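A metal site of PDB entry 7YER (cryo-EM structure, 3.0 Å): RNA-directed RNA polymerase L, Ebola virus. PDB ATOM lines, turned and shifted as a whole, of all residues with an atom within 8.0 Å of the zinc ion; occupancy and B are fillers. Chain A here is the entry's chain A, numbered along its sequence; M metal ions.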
ATOM      1  N   LYS A1140     -15.694  15.454 -15.160  1.00  0.00           N
ATOM      2  CA  LYS A1140     -14.321  15.100 -15.514  1.00  0.00           C
ATOM      3  C   LYS A1140     -13.555  16.383 -15.801  1.00  0.00           C
ATOM      4  O   LYS A1140     -13.935  17.144 -16.698  1.00  0.00           O
ATOM      5  CB  LYS A1140     -14.296  14.166 -16.723  1.00  0.00           C
ATOM      6  CG  LYS A1140     -12.927  13.971 -17.325  1.00  0.00           C
ATOM      7  CD  LYS A1140     -12.981  13.053 -18.542  1.00  0.00           C
ATOM      8  CE  LYS A1140     -11.590  12.766 -19.078  1.00  0.00           C
ATOM      9  NZ  LYS A1140     -10.727  12.110 -18.050  1.00  0.00           N
ATOM     10  N   VAL A1142     -10.322  18.798 -16.931  1.00  0.00           N
ATOM     11  CA  VAL A1142      -9.422  18.770 -18.068  1.00  0.00           C
ATOM     12  C   VAL A1142      -8.095  19.484 -17.814  1.00  0.00           C
ATOM     13  O   VAL A1142      -7.070  19.069 -18.382  1.00  0.00           O
ATOM     14  CB  VAL A1142     -10.102  19.343 -19.331  1.00  0.00           C
ATOM     15  CG1 VAL A1142      -9.243  19.128 -20.562  1.00  0.00           C
ATOM     16  CG2 VAL A1142     -11.473  18.705 -19.522  1.00  0.00           C
ATOM     17  N   LEU A1144      -6.818  22.818 -18.397  1.00  0.00           N
ATOM     18  CA  LEU A1144      -6.277  23.532 -19.543  1.00  0.00           C
ATOM     19  C   LEU A1144      -5.231  24.554 -19.107  1.00  0.00           C
ATOM     20  O   LEU A1144      -5.176  24.984 -17.958  1.00  0.00           O
ATOM     21  CB  LEU A1144      -7.393  24.228 -20.311  1.00  0.00           C
ATOM     22  CG  LEU A1144      -8.321  23.312 -21.103  1.00  0.00           C
ATOM     23  CD1 LEU A1144      -9.464  24.104 -21.702  1.00  0.00           C
ATOM     24  CD2 LEU A1144      -7.546  22.570 -22.179  1.00  0.00           C
ATOM     25  N   GLN A1149      -6.100  24.260 -26.257  1.00  0.00           N
ATOM     26  CA  GLN A1149      -7.521  24.149 -26.514  1.00  0.00           C
ATOM     27  C   GLN A1149      -8.017  22.811 -26.019  1.00  0.00           C
ATOM     28  O   GLN A1149      -7.303  21.809 -26.085  1.00  0.00           O
ATOM     29  CB  GLN A1149      -7.834  24.315 -28.009  1.00  0.00           C
ATOM     30  CG  GLN A1149      -7.708  25.740 -28.512  1.00  0.00           C
ATOM     31  CD  GLN A1149      -7.820  25.834 -30.021  1.00  0.00           C
ATOM     32  OE1 GLN A1149      -7.825  24.821 -30.720  1.00  0.00           O
ATOM     33  NE2 GLN A1149      -7.906  27.053 -30.535  1.00  0.00           N
ATOM     34  N   CYS A1150      -9.250  22.781 -25.510  1.00  0.00           N
ATOM     35  CA  CYS A1150      -9.793  21.578 -24.905  1.00  0.00           C
ATOM     36  C   CYS A1150     -10.040  20.516 -25.971  1.00  0.00           C
ATOM     37  O   CYS A1150     -10.782  20.780 -26.926  1.00  0.00           O
ATOM     38  CB  CYS A1150     -11.093  21.900 -24.170  1.00  0.00           C
ATOM     39  SG  CYS A1150     -11.721  20.559 -23.136  1.00  0.00           S
ATOM     40  N   PRO A1151      -9.435  19.335 -25.866  1.00  0.00           N
ATOM     41  CA  PRO A1151      -9.743  18.265 -26.837  1.00  0.00           C
ATOM     42  C   PRO A1151     -11.199  17.845 -26.819  1.00  0.00           C
ATOM     43  O   PRO A1151     -11.741  17.479 -27.873  1.00  0.00           O
ATOM     44  CB  PRO A1151      -8.811  17.115 -26.400  1.00  0.00           C
ATOM     45  CG  PRO A1151      -7.759  17.762 -25.559  1.00  0.00           C
ATOM     46  CD  PRO A1151      -8.414  18.919 -24.889  1.00  0.00           C
ATOM     47  N   GLN A1152     -11.856  17.871 -25.653  1.00  0.00           N
ATOM     48  CA  GLN A1152     -13.252  17.454 -25.579  1.00  0.00           C
ATOM     49  C   GLN A1152     -14.161  18.422 -26.322  1.00  0.00           C
ATOM     50  O   GLN A1152     -15.086  17.998 -27.033  1.00  0.00           O
ATOM     51  CB  GLN A1152     -13.678  17.337 -24.118  1.00  0.00           C
ATOM     52  CG  GLN A1152     -12.790  16.447 -23.281  1.00  0.00           C
ATOM     53  CD  GLN A1152     -13.393  15.082 -23.045  1.00  0.00           C
ATOM     54  OE1 GLN A1152     -14.610  14.926 -23.011  1.00  0.00           O
ATOM     55  NE2 GLN A1152     -12.540  14.077 -22.863  1.00  0.00           N
ATOM     56  N   CYS A1153     -13.922  19.732 -26.176  1.00  0.00           N
ATOM     57  CA  CYS A1153     -14.771  20.718 -26.830  1.00  0.00           C
ATOM     58  C   CYS A1153     -14.629  20.667 -28.348  1.00  0.00           C
ATOM     59  O   CYS A1153     -15.590  20.974 -29.074  1.00  0.00           O
ATOM     60  CB  CYS A1153     -14.462  22.117 -26.307  1.00  0.00           C
ATOM     61  SG  CYS A1153     -14.821  22.358 -24.548  1.00  0.00           S
ATOM     62  N   SER A1154     -13.447  20.314 -28.852  1.00  0.00           N
ATOM     63  CA  SER A1154     -13.260  20.204 -30.292  1.00  0.00           C
ATOM     64  C   SER A1154     -14.120  19.098 -30.888  1.00  0.00           C
ATOM     65  O   SER A1154     -14.698  19.261 -31.960  1.00  0.00           O
ATOM     66  CB  SER A1154     -11.777  19.963 -30.617  1.00  0.00           C
ATOM     67  OG  SER A1154     -11.306  18.778 -29.995  1.00  0.00           O
ATOM     68  N   LYS A1162     -21.466  19.172 -25.880  1.00  0.00           N
ATOM     69  CA  LYS A1162     -20.489  18.889 -24.824  1.00  0.00           C
ATOM     70  C   LYS A1162     -20.622  19.946 -23.745  1.00  0.00           C
ATOM     71  O   LYS A1162     -19.816  20.887 -23.665  1.00  0.00           O
ATOM     72  CB  LYS A1162     -19.065  18.850 -25.383  1.00  0.00           C
ATOM     73  CG  LYS A1162     -18.850  17.790 -26.452  1.00  0.00           C
ATOM     74  CD  LYS A1162     -18.517  16.435 -25.831  1.00  0.00           C
ATOM     75  CE  LYS A1162     -17.988  15.465 -26.869  1.00  0.00           C
ATOM     76  NZ  LYS A1162     -17.605  14.166 -26.268  1.00  0.00           N
ATOM     77  N   PRO A1163     -21.643  19.836 -22.890  1.00  0.00           N
ATOM     78  CA  PRO A1163     -21.797  20.816 -21.804  1.00  0.00           C
ATOM     79  C   PRO A1163     -20.660  20.706 -20.802  1.00  0.00           C
ATOM     80  O   PRO A1163     -20.101  19.629 -20.579  1.00  0.00           O
ATOM     81  CB  PRO A1163     -23.137  20.435 -21.168  1.00  0.00           C
ATOM     82  CG  PRO A1163     -23.791  19.487 -22.135  1.00  0.00           C
ATOM     83  CD  PRO A1163     -22.694  18.810 -22.856  1.00  0.00           C
ATOM     84  N   PHE A1164     -20.316  21.840 -20.199  1.00  0.00           N
ATOM     85  CA  PHE A1164     -19.236  21.856 -19.221  1.00  0.00           C
ATOM     86  C   PHE A1164     -19.366  23.073 -18.322  1.00  0.00           C
ATOM     87  O   PHE A1164     -20.093  24.026 -18.620  1.00  0.00           O
ATOM     88  CB  PHE A1164     -17.861  21.856 -19.914  1.00  0.00           C
ATOM     89  CG  PHE A1164     -17.626  23.018 -20.824  1.00  0.00           C
ATOM     90  CD1 PHE A1164     -17.076  24.196 -20.331  1.00  0.00           C
ATOM     91  CD2 PHE A1164     -17.934  22.946 -22.173  1.00  0.00           C
ATOM     92  CE1 PHE A1164     -16.852  25.272 -21.165  1.00  0.00           C
ATOM     93  CE2 PHE A1164     -17.706  24.013 -23.006  1.00  0.00           C
ATOM     94  CZ  PHE A1164     -17.163  25.177 -22.507  1.00  0.00           C
ATOM     95  N   VAL A1165     -18.649  23.017 -17.200  1.00  0.00           N
ATOM     96  CA  VAL A1165     -18.540  24.110 -16.250  1.00  0.00           C
ATOM     97  C   VAL A1165     -17.133  24.687 -16.351  1.00  0.00           C
ATOM     98  O   VAL A1165     -16.157  23.945 -16.447  1.00  0.00           O
ATOM     99  CB  VAL A1165     -18.826  23.634 -14.805  1.00  0.00           C
ATOM    100  CG1 VAL A1165     -18.850  24.809 -13.847  1.00  0.00           C
ATOM    101  CG2 VAL A1165     -20.145  22.870 -14.759  1.00  0.00           C
ATOM    102  N   ALA A1344      -9.969  25.733 -16.060  1.00  0.00           N
ATOM    103  CA  ALA A1344     -10.327  24.332 -16.011  1.00  0.00           C
ATOM    104  C   ALA A1344     -11.735  24.116 -16.561  1.00  0.00           C
ATOM    105  O   ALA A1344     -12.619  24.958 -16.379  1.00  0.00           O
ATOM    106  CB  ALA A1344     -10.252  23.785 -14.582  1.00  0.00           C
ATOM    107  N   HIS A1345     -11.915  22.976 -17.230  1.00  0.00           N
ATOM    108  CA  HIS A1345     -13.200  22.561 -17.790  1.00  0.00           C
ATOM    109  C   HIS A1345     -13.679  21.312 -17.078  1.00  0.00           C
ATOM    110  O   HIS A1345     -12.950  20.311 -17.009  1.00  0.00           O
ATOM    111  CB  HIS A1345     -13.081  22.288 -19.290  1.00  0.00           C
ATOM    112  CG  HIS A1345     -13.160  23.516 -20.145  1.00  0.00           C
ATOM    113  ND1 HIS A1345     -13.277  23.445 -21.517  1.00  0.00           N
ATOM    114  CD2 HIS A1345     -13.130  24.832 -19.832  1.00  0.00           C
ATOM    115  CE1 HIS A1345     -13.318  24.677 -22.012  1.00  0.00           C
ATOM    116  NE2 HIS A1345     -13.236  25.529 -21.004  1.00  0.00           N
ATOM    117  N   LEU A1346     -14.893  21.349 -16.556  1.00  0.00           N
ATOM    118  CA  LEU A1346     -15.543  20.183 -15.948  1.00  0.00           C
ATOM    119  C   LEU A1346     -16.590  19.690 -16.937  1.00  0.00           C
ATOM    120  O   LEU A1346     -17.662  20.282 -17.051  1.00  0.00           O
ATOM    121  CB  LEU A1346     -16.163  20.540 -14.603  1.00  0.00           C
ATOM    122  CG  LEU A1346     -15.241  20.630 -13.380  1.00  0.00           C
ATOM    123  CD1 LEU A1346     -14.594  21.998 -13.298  1.00  0.00           C
ATOM    124  CD2 LEU A1346     -16.032  20.334 -12.117  1.00  0.00           C
ATOM    125  N   HIS A1347     -16.267  18.613 -17.643  1.00  0.00           N
ATOM    126  CA  HIS A1347     -17.142  18.054 -18.668  1.00  0.00           C
ATOM    127  C   HIS A1347     -17.916  16.869 -18.087  1.00  0.00           C
ATOM    128  O   HIS A1347     -17.305  15.930 -17.564  1.00  0.00           O
ATOM    129  CB  HIS A1347     -16.341  17.599 -19.885  1.00  0.00           C
ATOM    130  CG  HIS A1347     -15.858  18.720 -20.755  1.00  0.00           C
ATOM    131  ND1 HIS A1347     -16.595  19.210 -21.811  1.00  0.00           N
ATOM    132  CD2 HIS A1347     -14.723  19.447 -20.725  1.00  0.00           C
ATOM    133  CE1 HIS A1347     -15.927  20.186 -22.394  1.00  0.00           C
ATOM    134  NE2 HIS A1347     -14.787  20.360 -21.757  1.00  0.00           N
HETATM  135 ZN    ZN M   1     -13.619  21.777 -22.674  1.00  0.00          ZN
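The nearest printed residue that does not touch the zinc ion is Phe 1164 (4.5 Å).
N of His 1347 lies within hydrogen-bond range of O of Lys 1140. The backbone carbonyl oxygen of His 1345 is in hydrogen-bond range of the backbone NH of Val 1142 (3.0 Å). The side-chain sulfur of Cys 1150 sits close to the backbone NH of Gln 1152, 3.7 Å away.
The zinc ion is bound by NE2 of His 1347, at 2.1 Å. ND1 of His 1345 binds the zinc ion (2.1 Å). SG of Cys 1153 is bound to the zinc ion (2.3 Å). The zinc ion is bound by SG of Cys 1150 (2.3 Å). The zinc ion has four donor atoms within binding distance.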
